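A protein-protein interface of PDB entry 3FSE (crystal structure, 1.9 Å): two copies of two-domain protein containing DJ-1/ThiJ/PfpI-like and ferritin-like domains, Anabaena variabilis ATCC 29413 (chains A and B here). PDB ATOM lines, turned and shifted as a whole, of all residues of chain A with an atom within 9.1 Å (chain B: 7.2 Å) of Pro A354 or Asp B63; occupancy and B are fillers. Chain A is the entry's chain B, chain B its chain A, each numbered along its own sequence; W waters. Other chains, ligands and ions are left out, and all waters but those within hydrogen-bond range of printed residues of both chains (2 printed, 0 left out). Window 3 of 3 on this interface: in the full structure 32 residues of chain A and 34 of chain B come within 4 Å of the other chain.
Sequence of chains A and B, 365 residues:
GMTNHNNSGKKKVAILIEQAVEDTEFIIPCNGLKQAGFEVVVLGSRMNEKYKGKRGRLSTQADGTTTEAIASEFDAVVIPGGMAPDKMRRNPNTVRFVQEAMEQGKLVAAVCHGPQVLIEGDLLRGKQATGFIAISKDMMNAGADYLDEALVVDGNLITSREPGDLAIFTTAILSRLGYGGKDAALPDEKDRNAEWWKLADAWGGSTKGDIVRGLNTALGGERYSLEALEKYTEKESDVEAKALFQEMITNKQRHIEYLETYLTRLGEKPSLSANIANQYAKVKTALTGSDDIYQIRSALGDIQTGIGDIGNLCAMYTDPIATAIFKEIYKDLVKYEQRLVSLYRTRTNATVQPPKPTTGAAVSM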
ATOM      1  N   ILE A 293      -2.583  16.399   0.503  1.00  0.00           N
ATOM      2  CA  ILE A 293      -3.984  16.790   0.661  1.00  0.00           C
ATOM      3  C   ILE A 293      -4.492  16.549   2.112  1.00  0.00           C
ATOM      4  O   ILE A 293      -5.301  17.340   2.622  1.00  0.00           O
ATOM      5  CB  ILE A 293      -4.879  16.128  -0.408  1.00  0.00           C
ATOM      6  CG1 ILE A 293      -4.472  16.599  -1.811  1.00  0.00           C
ATOM      7  CG2 ILE A 293      -6.318  16.479  -0.203  1.00  0.00           C
ATOM      8  CD1 ILE A 293      -5.143  15.820  -2.929  1.00  0.00           C
ATOM      9  N   TYR A 294      -4.016  15.490   2.775  1.00  0.00           N
ATOM     10  CA  TYR A 294      -4.452  15.204   4.157  1.00  0.00           C
ATOM     11  C   TYR A 294      -4.030  16.298   5.166  1.00  0.00           C
ATOM     12  O   TYR A 294      -4.762  16.577   6.132  1.00  0.00           O
ATOM     13  CB  TYR A 294      -3.965  13.844   4.619  1.00  0.00           C
ATOM     14  CG  TYR A 294      -4.701  13.331   5.825  1.00  0.00           C
ATOM     15  CD1 TYR A 294      -5.869  12.567   5.681  1.00  0.00           C
ATOM     16  CD2 TYR A 294      -4.233  13.589   7.119  1.00  0.00           C
ATOM     17  CE1 TYR A 294      -6.556  12.076   6.805  1.00  0.00           C
ATOM     18  CE2 TYR A 294      -4.909  13.109   8.241  1.00  0.00           C
ATOM     19  CZ  TYR A 294      -6.067  12.358   8.083  1.00  0.00           C
ATOM     20  OH  TYR A 294      -6.707  11.906   9.204  1.00  0.00           O
ATOM     21  N   ILE A 296      -3.786  19.447   4.416  1.00  0.00           N
ATOM     22  CA  ILE A 296      -4.703  20.575   4.143  1.00  0.00           C
ATOM     23  C   ILE A 296      -6.054  20.352   4.846  1.00  0.00           C
ATOM     24  O   ILE A 296      -6.572  21.275   5.464  1.00  0.00           O
ATOM     25  CB  ILE A 296      -4.946  20.814   2.608  1.00  0.00           C
ATOM     26  CG1 ILE A 296      -3.647  21.160   1.857  1.00  0.00           C
ATOM     27  CG2 ILE A 296      -5.930  21.960   2.380  1.00  0.00           C
ATOM     28  CD1 ILE A 296      -3.831  21.118   0.293  1.00  0.00           C
ATOM     29  N   ARG A 297      -6.608  19.135   4.735  1.00  0.00           N
ATOM     30  CA  ARG A 297      -7.864  18.766   5.442  1.00  0.00           C
ATOM     31  C   ARG A 297      -7.737  18.938   6.947  1.00  0.00           C
ATOM     32  O   ARG A 297      -8.683  19.369   7.587  1.00  0.00           O
ATOM     33  CB  ARG A 297      -8.261  17.301   5.211  1.00  0.00           C
ATOM     34  CG  ARG A 297      -9.082  17.033   4.016  1.00  0.00           C
ATOM     35  CD  ARG A 297      -9.474  15.516   3.958  1.00  0.00           C
ATOM     36  NE  ARG A 297     -10.580  15.158   4.860  1.00  0.00           N
ATOM     37  CZ  ARG A 297     -10.972  13.910   5.127  1.00  0.00           C
ATOM     38  NH1 ARG A 297     -10.316  12.853   4.646  1.00  0.00           N
ATOM     39  NH2 ARG A 297     -12.015  13.714   5.936  1.00  0.00           N
ATOM     40  N   SER A 298      -6.582  18.542   7.494  1.00  0.00           N
ATOM     41  CA  SER A 298      -6.290  18.654   8.920  1.00  0.00           C
ATOM     42  C   SER A 298      -6.236  20.118   9.365  1.00  0.00           C
ATOM     43  O   SER A 298      -6.871  20.505  10.351  1.00  0.00           O
ATOM     44  CB  SER A 298      -4.976  17.956   9.257  1.00  0.00           C
ATOM     45  OG  SER A 298      -4.989  16.593   8.828  1.00  0.00           O
ATOM     46  N   ALA A 299      -5.496  20.922   8.608  1.00  0.00           N
ATOM     47  CA  ALA A 299      -5.367  22.347   8.878  1.00  0.00           C
ATOM     48  C   ALA A 299      -6.718  23.065   8.757  1.00  0.00           C
ATOM     49  O   ALA A 299      -6.996  23.961   9.528  1.00  0.00           O
ATOM     50  CB  ALA A 299      -4.332  22.982   7.972  1.00  0.00           C
ATOM     51  N   LEU A 300      -7.534  22.666   7.784  1.00  0.00           N
ATOM     52  CA  LEU A 300      -8.859  23.260   7.606  1.00  0.00           C
ATOM     53  C   LEU A 300      -9.740  22.885   8.792  1.00  0.00           C
ATOM     54  O   LEU A 300     -10.412  23.744   9.345  1.00  0.00           O
ATOM     55  CB  LEU A 300      -9.497  22.828   6.298  1.00  0.00           C
ATOM     56  CG  LEU A 300     -10.864  23.397   5.926  1.00  0.00           C
ATOM     57  CD1 LEU A 300     -10.905  24.945   6.051  1.00  0.00           C
ATOM     58  CD2 LEU A 300     -11.218  22.900   4.510  1.00  0.00           C
ATOM     59  N   GLY A 301      -9.714  21.617   9.211  1.00  0.00           N
ATOM     60  CA  GLY A 301     -10.447  21.218  10.414  1.00  0.00           C
ATOM     61  C   GLY A 301     -10.002  21.959  11.671  1.00  0.00           C
ATOM     62  O   GLY A 301     -10.837  22.371  12.464  1.00  0.00           O
ATOM     63  N   GLN A 304     -11.433  25.481  11.682  1.00  0.00           N
ATOM     64  CA  GLN A 304     -12.859  25.446  12.062  1.00  0.00           C
ATOM     65  C   GLN A 304     -13.031  25.231  13.583  1.00  0.00           C
ATOM     66  O   GLN A 304     -13.916  25.830  14.182  1.00  0.00           O
ATOM     67  CB  GLN A 304     -13.655  24.440  11.261  1.00  0.00           C
ATOM     68  CG  GLN A 304     -13.733  24.810   9.748  1.00  0.00           C
ATOM     69  CD  GLN A 304     -14.717  23.983   8.965  1.00  0.00           C
ATOM     70  OE1 GLN A 304     -15.279  24.454   7.962  1.00  0.00           O
ATOM     71  NE2 GLN A 304     -14.936  22.757   9.393  1.00  0.00           N
ATOM     72  N   VAL A 341      -9.647  26.497   2.123  1.00  0.00           N
ATOM     73  CA  VAL A 341     -10.681  25.797   1.324  1.00  0.00           C
ATOM     74  C   VAL A 341     -10.416  26.001  -0.178  1.00  0.00           C
ATOM     75  O   VAL A 341     -10.541  25.046  -0.948  1.00  0.00           O
ATOM     76  CB  VAL A 341     -12.147  26.102   1.759  1.00  0.00           C
ATOM     77  CG1 VAL A 341     -12.630  27.485   1.282  1.00  0.00           C
ATOM     78  CG2 VAL A 341     -13.088  24.989   1.265  1.00  0.00           C
ATOM     79  N   TYR A 344      -7.429  23.798  -0.983  1.00  0.00           N
ATOM     80  CA  TYR A 344      -7.925  22.424  -0.874  1.00  0.00           C
ATOM     81  C   TYR A 344      -8.702  21.966  -2.103  1.00  0.00           C
ATOM     82  O   TYR A 344      -8.506  20.832  -2.548  1.00  0.00           O
ATOM     83  CB  TYR A 344      -8.762  22.282   0.399  1.00  0.00           C
ATOM     84  CG  TYR A 344      -9.337  20.915   0.678  1.00  0.00           C
ATOM     85  CD1 TYR A 344      -8.614  19.731   0.415  1.00  0.00           C
ATOM     86  CD2 TYR A 344     -10.595  20.801   1.284  1.00  0.00           C
ATOM     87  CE1 TYR A 344      -9.171  18.476   0.692  1.00  0.00           C
ATOM     88  CE2 TYR A 344     -11.140  19.565   1.584  1.00  0.00           C
ATOM     89  CZ  TYR A 344     -10.433  18.402   1.283  1.00  0.00           C
ATOM     90  OH  TYR A 344     -10.968  17.166   1.572  1.00  0.00           O
ATOM     91  N   THR A 348      -7.365  18.815  -4.844  1.00  0.00           N
ATOM     92  CA  THR A 348      -8.160  17.576  -4.915  1.00  0.00           C
ATOM     93  C   THR A 348      -8.766  17.336  -6.308  1.00  0.00           C
ATOM     94  O   THR A 348      -9.563  18.154  -6.795  1.00  0.00           O
ATOM     95  CB  THR A 348      -9.323  17.549  -3.876  1.00  0.00           C
ATOM     96  OG1 THR A 348      -8.833  17.882  -2.564  1.00  0.00           O
ATOM     97  CG2 THR A 348      -9.988  16.160  -3.838  1.00  0.00           C
ATOM     98  N   THR A 351     -14.318  14.678  -5.382  1.00  0.00           N
ATOM     99  CA  THR A 351     -15.209  15.311  -4.402  1.00  0.00           C
ATOM    100  C   THR A 351     -14.391  15.531  -3.123  1.00  0.00           C
ATOM    101  O   THR A 351     -13.827  14.584  -2.580  1.00  0.00           O
ATOM    102  CB  THR A 351     -16.478  14.458  -4.100  1.00  0.00           C
ATOM    103  OG1 THR A 351     -17.336  14.478  -5.246  1.00  0.00           O
ATOM    104  CG2 THR A 351     -17.260  15.013  -2.904  1.00  0.00           C
ATOM    105  N   VAL A 352     -14.311  16.787  -2.686  1.00  0.00           N
ATOM    106  CA  VAL A 352     -13.532  17.146  -1.513  1.00  0.00           C
ATOM    107  C   VAL A 352     -14.173  16.540  -0.262  1.00  0.00           C
ATOM    108  O   VAL A 352     -15.406  16.572  -0.095  1.00  0.00           O
ATOM    109  CB  VAL A 352     -13.333  18.687  -1.357  1.00  0.00           C
ATOM    110  CG1 VAL A 352     -12.597  19.270  -2.572  1.00  0.00           C
ATOM    111  CG2 VAL A 352     -14.647  19.423  -1.128  1.00  0.00           C
ATOM    112  N   GLN A 353     -13.337  15.949   0.586  1.00  0.00           N
ATOM    113  CA  GLN A 353     -13.815  15.375   1.828  1.00  0.00           C
ATOM    114  C   GLN A 353     -13.999  16.503   2.831  1.00  0.00           C
ATOM    115  O   GLN A 353     -13.398  17.568   2.682  1.00  0.00           O
ATOM    116  CB  GLN A 353     -12.863  14.291   2.355  1.00  0.00           C
ATOM    117  CG  GLN A 353     -12.731  13.124   1.402  1.00  0.00           C
ATOM    118  CD  GLN A 353     -14.084  12.549   1.102  1.00  0.00           C
ATOM    119  OE1 GLN A 353     -14.703  11.913   1.957  1.00  0.00           O
ATOM    120  NE2 GLN A 353     -14.596  12.844  -0.090  1.00  0.00           N
ATOM    121  N   PRO A 354     -14.854  16.291   3.843  1.00  0.00           N
ATOM    122  CA  PRO A 354     -15.023  17.350   4.830  1.00  0.00           C
ATOM    123  C   PRO A 354     -13.715  17.659   5.580  1.00  0.00           C
ATOM    124  O   PRO A 354     -12.798  16.852   5.543  1.00  0.00           O
ATOM    125  CB  PRO A 354     -16.047  16.763   5.800  1.00  0.00           C
ATOM    126  CG  PRO A 354     -16.753  15.720   5.037  1.00  0.00           C
ATOM    127  CD  PRO A 354     -15.736  15.140   4.127  1.00  0.00           C
ATOM    128  N   PRO A 355     -13.615  18.829   6.215  1.00  0.00           N
ATOM    129  CA  PRO A 355     -12.464  19.138   7.062  1.00  0.00           C
ATOM    130  C   PRO A 355     -12.283  18.054   8.147  1.00  0.00           C
ATOM    131  O   PRO A 355     -13.285  17.468   8.585  1.00  0.00           O
ATOM    132  CB  PRO A 355     -12.880  20.473   7.691  1.00  0.00           C
ATOM    133  CG  PRO A 355     -13.782  21.077   6.685  1.00  0.00           C
ATOM    134  CD  PRO A 355     -14.562  19.964   6.155  1.00  0.00           C
ATOM    135  N   LYS A 356     -11.042  17.755   8.532  1.00  0.00           N
ATOM    136  CA  LYS A 356     -10.779  16.727   9.535  1.00  0.00           C
ATOM    137  C   LYS A 356     -10.038  17.309  10.760  1.00  0.00           C
ATOM    138  O   LYS A 356      -8.804  17.280  10.805  1.00  0.00           O
ATOM    139  CB  LYS A 356     -10.046  15.544   8.913  1.00  0.00           C
ATOM    140  CG  LYS A 356     -10.087  14.317   9.802  1.00  0.00           C
ATOM    141  CD  LYS A 356      -9.800  13.060   9.050  1.00  0.00           C
ATOM    142  CE  LYS A 356      -9.754  11.876   9.998  1.00  0.00           C
ATOM    143  NZ  LYS A 356      -9.298  10.627   9.318  1.00  0.00           N
ATOM    144  N   PRO A 357     -10.792  17.854  11.745  1.00  0.00           N
ATOM    145  CA  PRO A 357     -10.137  18.437  12.937  1.00  0.00           C
ATOM    146  C   PRO A 357      -9.344  17.387  13.702  1.00  0.00           C
ATOM    147  O   PRO A 357      -9.749  16.210  13.750  1.00  0.00           O
ATOM    148  CB  PRO A 357     -11.309  19.010  13.757  1.00  0.00           C
ATOM    149  CG  PRO A 357     -12.523  18.354  13.222  1.00  0.00           C
ATOM    150  CD  PRO A 357     -12.255  18.021  11.806  1.00  0.00           C
ATOM    151  N   ILE B  15     -29.459  19.938   4.570  1.00  0.00           N
ATOM    152  CA  ILE B  15     -30.202  20.454   5.714  1.00  0.00           C
ATOM    153  C   ILE B  15     -29.172  21.130   6.583  1.00  0.00           C
ATOM    154  O   ILE B  15     -28.248  20.486   7.073  1.00  0.00           O
ATOM    155  CB  ILE B  15     -30.957  19.385   6.495  1.00  0.00           C
ATOM    156  CG1 ILE B  15     -31.809  18.560   5.527  1.00  0.00           C
ATOM    157  CG2 ILE B  15     -31.829  20.057   7.613  1.00  0.00           C
ATOM    158  CD1 ILE B  15     -32.751  17.594   6.210  1.00  0.00           C
ATOM    159  N   ILE B  17     -27.648  22.899   9.876  1.00  0.00           N
ATOM    160  CA  ILE B  17     -27.777  22.743  11.311  1.00  0.00           C
ATOM    161  C   ILE B  17     -26.812  23.677  12.049  1.00  0.00           C
ATOM    162  O   ILE B  17     -25.750  24.059  11.528  1.00  0.00           O
ATOM    163  CB  ILE B  17     -27.559  21.271  11.755  1.00  0.00           C
ATOM    164  CG1 ILE B  17     -28.146  21.020  13.172  1.00  0.00           C
ATOM    165  CG2 ILE B  17     -26.091  20.861  11.652  1.00  0.00           C
ATOM    166  CD1 ILE B  17     -28.126  19.567  13.608  1.00  0.00           C
ATOM    167  N   PHE B  26     -35.657  20.361  12.360  1.00  0.00           N
ATOM    168  CA  PHE B  26     -34.606  19.582  11.724  1.00  0.00           C
ATOM    169  C   PHE B  26     -35.085  18.132  11.459  1.00  0.00           C
ATOM    170  O   PHE B  26     -34.967  17.629  10.336  1.00  0.00           O
ATOM    171  CB  PHE B  26     -33.332  19.594  12.580  1.00  0.00           C
ATOM    172  CG  PHE B  26     -32.223  18.736  12.017  1.00  0.00           C
ATOM    173  CD1 PHE B  26     -32.096  17.414  12.404  1.00  0.00           C
ATOM    174  CD2 PHE B  26     -31.352  19.243  11.047  1.00  0.00           C
ATOM    175  CE1 PHE B  26     -31.100  16.604  11.845  1.00  0.00           C
ATOM    176  CE2 PHE B  26     -30.360  18.432  10.479  1.00  0.00           C
ATOM    177  CZ  PHE B  26     -30.225  17.136  10.882  1.00  0.00           C
ATOM    178  N   VAL B  40     -29.634  12.869   2.031  1.00  0.00           N
ATOM    179  CA  VAL B  40     -29.647  14.049   2.901  1.00  0.00           C
ATOM    180  C   VAL B  40     -28.242  14.248   3.492  1.00  0.00           C
ATOM    181  O   VAL B  40     -27.647  13.322   4.055  1.00  0.00           O
ATOM    182  CB  VAL B  40     -30.719  13.974   4.005  1.00  0.00           C
ATOM    183  CG1 VAL B  40     -30.656  15.207   4.904  1.00  0.00           C
ATOM    184  CG2 VAL B  40     -32.094  13.870   3.388  1.00  0.00           C
ATOM    185  N   VAL B  41     -27.721  15.456   3.313  1.00  0.00           N
ATOM    186  CA  VAL B  41     -26.422  15.876   3.793  1.00  0.00           C
ATOM    187  C   VAL B  41     -26.665  16.964   4.842  1.00  0.00           C
ATOM    188  O   VAL B  41     -27.236  18.018   4.540  1.00  0.00           O
ATOM    189  CB  VAL B  41     -25.551  16.396   2.651  1.00  0.00           C
ATOM    190  CG1 VAL B  41     -24.152  16.742   3.151  1.00  0.00           C
ATOM    191  CG2 VAL B  41     -25.462  15.344   1.520  1.00  0.00           C
ATOM    192  N   VAL B  42     -26.275  16.686   6.076  1.00  0.00           N
ATOM    193  CA  VAL B  42     -26.428  17.638   7.174  1.00  0.00           C
ATOM    194  C   VAL B  42     -25.187  18.532   7.156  1.00  0.00           C
ATOM    195  O   VAL B  42     -24.076  18.035   7.321  1.00  0.00           O
ATOM    196  CB  VAL B  42     -26.551  16.921   8.496  1.00  0.00           C
ATOM    197  CG1 VAL B  42     -26.596  17.958   9.668  1.00  0.00           C
ATOM    198  CG2 VAL B  42     -27.801  15.965   8.464  1.00  0.00           C
ATOM    199  N   LEU B  43     -25.381  19.830   6.917  1.00  0.00           N
ATOM    200  CA  LEU B  43     -24.290  20.786   6.833  1.00  0.00           C
ATOM    201  C   LEU B  43     -24.255  21.702   8.041  1.00  0.00           C
ATOM    202  O   LEU B  43     -25.156  22.523   8.234  1.00  0.00           O
ATOM    203  CB  LEU B  43     -24.411  21.629   5.565  1.00  0.00           C
ATOM    204  CG  LEU B  43     -24.327  20.881   4.238  1.00  0.00           C
ATOM    205  CD1 LEU B  43     -24.518  21.855   3.070  1.00  0.00           C
ATOM    206  CD2 LEU B  43     -22.993  20.124   4.106  1.00  0.00           C
ATOM    207  N   GLY B  44     -23.209  21.543   8.858  1.00  0.00           N
ATOM    208  CA  GLY B  44     -22.963  22.405   9.979  1.00  0.00           C
ATOM    209  C   GLY B  44     -21.879  23.425   9.644  1.00  0.00           C
ATOM    210  O   GLY B  44     -21.524  23.665   8.469  1.00  0.00           O
ATOM    211  N   ARG B  46     -18.951  23.079  11.473  1.00  0.00           N
ATOM    212  CA  ARG B  46     -17.744  22.268  11.631  1.00  0.00           C
ATOM    213  C   ARG B  46     -18.034  20.803  11.930  1.00  0.00           C
ATOM    214  O   ARG B  46     -19.159  20.439  12.296  1.00  0.00           O
ATOM    215  CB  ARG B  46     -16.828  22.886  12.692  1.00  0.00           C
ATOM    216  CG  ARG B  46     -17.442  23.100  14.066  1.00  0.00           C
ATOM    217  CD  ARG B  46     -16.672  24.158  14.877  1.00  0.00           C
ATOM    218  NE  ARG B  46     -16.874  25.502  14.307  1.00  0.00           N
ATOM    219  CZ  ARG B  46     -17.881  26.331  14.590  1.00  0.00           C
ATOM    220  NH1 ARG B  46     -18.821  26.025  15.481  1.00  0.00           N
ATOM    221  NH2 ARG B  46     -17.941  27.514  13.981  1.00  0.00           N
ATOM    222  N   MET B  47     -17.013  19.976  11.738  1.00  0.00           N
ATOM    223  CA  MET B  47     -17.084  18.527  11.957  1.00  0.00           C
ATOM    224  C   MET B  47     -16.764  18.246  13.410  1.00  0.00           C
ATOM    225  O   MET B  47     -16.243  19.119  14.131  1.00  0.00           O
ATOM    226  CB  MET B  47     -16.129  17.809  11.011  1.00  0.00           C
ATOM    227  CG  MET B  47     -16.379  18.104   9.534  1.00  0.00           C
ATOM    228  SD  MET B  47     -18.161  17.619   8.881  1.00  0.00           S
ATOM    229  CE  MET B  47     -17.860  15.673   8.760  1.00  0.00           C
ATOM    230  N   TYR B  51     -24.258  18.799  17.464  1.00  0.00           N
ATOM    231  CA  TYR B  51     -25.278  19.853  17.424  1.00  0.00           C
ATOM    232  C   TYR B  51     -26.458  19.361  18.230  1.00  0.00           C
ATOM    233  O   TYR B  51     -26.996  18.277  17.947  1.00  0.00           O
ATOM    234  CB  TYR B  51     -25.686  20.190  15.993  1.00  0.00           C
ATOM    235  CG  TYR B  51     -24.553  20.864  15.287  1.00  0.00           C
ATOM    236  CD1 TYR B  51     -24.271  22.219  15.536  1.00  0.00           C
ATOM    237  CD2 TYR B  51     -23.743  20.173  14.404  1.00  0.00           C
ATOM    238  CE1 TYR B  51     -23.205  22.870  14.902  1.00  0.00           C
ATOM    239  CE2 TYR B  51     -22.660  20.813  13.775  1.00  0.00           C
ATOM    240  CZ  TYR B  51     -22.409  22.169  14.021  1.00  0.00           C
ATOM    241  OH  TYR B  51     -21.352  22.818  13.419  1.00  0.00           O
ATOM    242  N   THR B  60     -26.745  15.475  16.923  1.00  0.00           N
ATOM    243  CA  THR B  60     -26.116  14.889  15.753  1.00  0.00           C
ATOM    244  C   THR B  60     -24.874  15.644  15.308  1.00  0.00           C
ATOM    245  O   THR B  60     -24.750  16.845  15.537  1.00  0.00           O
ATOM    246  CB  THR B  60     -27.142  14.787  14.584  1.00  0.00           C
ATOM    247  OG1 THR B  60     -26.587  13.990  13.526  1.00  0.00           O
ATOM    248  CG2 THR B  60     -27.530  16.143  14.054  1.00  0.00           C
ATOM    249  N   GLN B  61     -23.958  14.922  14.676  1.00  0.00           N
ATOM    250  CA  GLN B  61     -22.796  15.537  14.073  1.00  0.00           C
ATOM    251  C   GLN B  61     -23.156  15.831  12.608  1.00  0.00           C
ATOM    252  O   GLN B  61     -24.107  15.258  12.070  1.00  0.00           O
ATOM    253  CB  GLN B  61     -21.553  14.653  14.219  1.00  0.00           C
ATOM    254  CG  GLN B  61     -21.148  14.467  15.698  1.00  0.00           C
ATOM    255  CD  GLN B  61     -19.685  14.127  15.909  1.00  0.00           C
ATOM    256  OE1 GLN B  61     -18.970  13.763  14.972  1.00  0.00           O
ATOM    257  NE2 GLN B  61     -19.224  14.254  17.148  1.00  0.00           N
ATOM    258  N   ALA B  62     -22.427  16.774  12.005  1.00  0.00           N
ATOM    259  CA  ALA B  62     -22.617  17.136  10.606  1.00  0.00           C
ATOM    260  C   ALA B  62     -21.964  16.091   9.714  1.00  0.00           C
ATOM    261  O   ALA B  62     -21.006  15.419  10.128  1.00  0.00           O
ATOM    262  CB  ALA B  62     -21.992  18.492  10.305  1.00  0.00           C
ATOM    263  N   ASP B  63     -22.501  15.977   8.506  1.00  0.00           N
ATOM    264  CA  ASP B  63     -21.929  15.148   7.416  1.00  0.00           C
ATOM    265  C   ASP B  63     -20.893  15.984   6.642  1.00  0.00           C
ATOM    266  O   ASP B  63     -19.986  15.445   6.008  1.00  0.00           O
ATOM    267  CB  ASP B  63     -23.004  14.763   6.414  1.00  0.00           C
ATOM    268  CG  ASP B  63     -24.089  13.901   7.021  1.00  0.00           C
ATOM    269  OD1 ASP B  63     -23.748  12.915   7.688  1.00  0.00           O
ATOM    270  OD2 ASP B  63     -25.281  14.213   6.811  1.00  0.00           O
ATOM    271  N   GLY B  64     -21.079  17.308   6.651  1.00  0.00           N
ATOM    272  CA  GLY B  64     -20.178  18.224   5.972  1.00  0.00           C
ATOM    273  C   GLY B  64     -20.373  19.598   6.555  1.00  0.00           C
ATOM    274  O   GLY B  64     -21.128  19.760   7.534  1.00  0.00           O
ATOM    275  N   THR B  65     -19.656  20.565   6.011  1.00  0.00           N
ATOM    276  CA  THR B  65     -19.820  21.959   6.424  1.00  0.00           C
ATOM    277  C   THR B  65     -20.138  22.825   5.215  1.00  0.00           C
ATOM    278  O   THR B  65     -19.872  22.455   4.067  1.00  0.00           O
ATOM    279  CB  THR B  65     -18.644  22.519   7.257  1.00  0.00           C
ATOM    280  OG1 THR B  65     -17.613  23.101   6.431  1.00  0.00           O
ATOM    281  CG2 THR B  65     -18.062  21.466   8.185  1.00  0.00           C
ATOM    282  N   GLU B  68     -16.905  23.895   2.591  1.00  0.00           N
ATOM    283  CA  GLU B  68     -16.571  23.092   1.396  1.00  0.00           C
ATOM    284  C   GLU B  68     -17.741  22.668   0.529  1.00  0.00           C
ATOM    285  O   GLU B  68     -17.510  22.218  -0.598  1.00  0.00           O
ATOM    286  CB  GLU B  68     -15.717  21.848   1.740  1.00  0.00           C
ATOM    287  CG  GLU B  68     -16.436  20.606   2.304  1.00  0.00           C
ATOM    288  CD  GLU B  68     -16.993  20.785   3.692  1.00  0.00           C
ATOM    289  OE1 GLU B  68     -16.749  21.844   4.347  1.00  0.00           O
ATOM    290  OE2 GLU B  68     -17.713  19.865   4.122  1.00  0.00           O
HETATM  291  O   HOH W   1     -14.303  20.789  11.214  1.00  0.00           O
HETATM  292  O   HOH W   2     -13.786  21.581  13.920  1.00  0.00           O
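Water W1 bridges the side-chain amide nitrogen (NE2) of Gln A304 (2.8 Å) and the backbone NH (N) of Met B47 (2.9 Å).
Water W2 bridges the backbone carbonyl oxygen (O) of Gly A301 (3.4 Å) and the backbone carbonyl oxygen (O) of Met B47 (3.5 Å).
O of Gln A304 sits at hydrogen-bond distance from NE of Arg B46 (3.0 Å).
OE1 of Gln A304 lies within hydrogen-bond range of OG1 of Thr B65 (3.1 Å).
Val A341 touches Glu B68 (CG2 to CA, 3.97 Å).
CB of Glu B68 touches CG2 of Val A352 (3.9 Å).
Met B47 touches Pro A354 (CE to CB, 3.6 Å).
O of Asp B63 touches CG of Pro A354, 3.4 Å away.
CA of Pro A354 touches OE2 of Glu B68 (3.8 Å).
O of Pro A355 touches CG of Met B47, at 3.3 Å.
Glu B68 touches Pro A355.
Met B47 touches Pro A357 (O to CG, 3.9 Å).
Of the printed residues of chain B, Gln A304 touches Arg B46 and Thr B65.
Of the printed residues of chain B, Val A341 touches Glu B68 (3.97 Å).
Thr A351 touches none of the printed residues of chain B.
Printed residues of chain B within 4 Å of Val A352: Glu B68.
Pro A354 touches three residues of chain B.
No residue of chain A comes within 4 Å of Val B42.
Printed residues of chain A within 4 Å of Met B47: Pro A354, Pro A355 and Pro A357.
No residue of chain A comes within 4 Å of Ala B62.
Of chain A, only Pro A354 comes within 4 Å of Asp B63.
Of the printed residues of chain A, Thr B65 touches Gln A304.
The nearest residue of chain B that does not touch Pro A354 is Gly B64 (4.3 Å).
The nearest residue of chain A that does not touch Asp B63 is Gln A353 (6.9 Å).
The backbone NH (N) of Val B42 is in hydrogen-bond range of the side-chain carboxylate (OD2) of Asp B63 (2.8 Å).
N of Arg B46 sits at hydrogen-bond distance from OH of Tyr B51 (3.1 Å).
The side-chain sulfur of Met B47 lies close to the backbone NH of Gly B64, at 3.7 Å.
OG1 of Thr B65 sits at hydrogen-bond distance from OE1 of Glu B68 (2.6 Å).
NE of Arg A297 sits at hydrogen-bond distance from O of Pro A354 (2.9 Å).
Printed residues of chain A that touch a printed residue of chain B: Gln A304, Val A341, Val A352, Pro A354, Pro A355 and Pro A357.
Hydrophobic or aromatic side chains of chain A within 4 Å of the printed part of chain B: Val A341, Val A352, Pro A354, Pro A355 and Pro A357.
Printed residues of chain B that touch a printed residue of chain A: Arg B46, Met B47, Asp B63, Thr B65 and Glu B68.
Hydrophobic or aromatic side chains of chain B that line the printed part of chain A: Met B47.
Among the printed residues, no Asp or Glu carboxylate lies within 4 Å of a Lys or Arg side-chain nitrogen of the other chain.
No position is printed for both chains.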
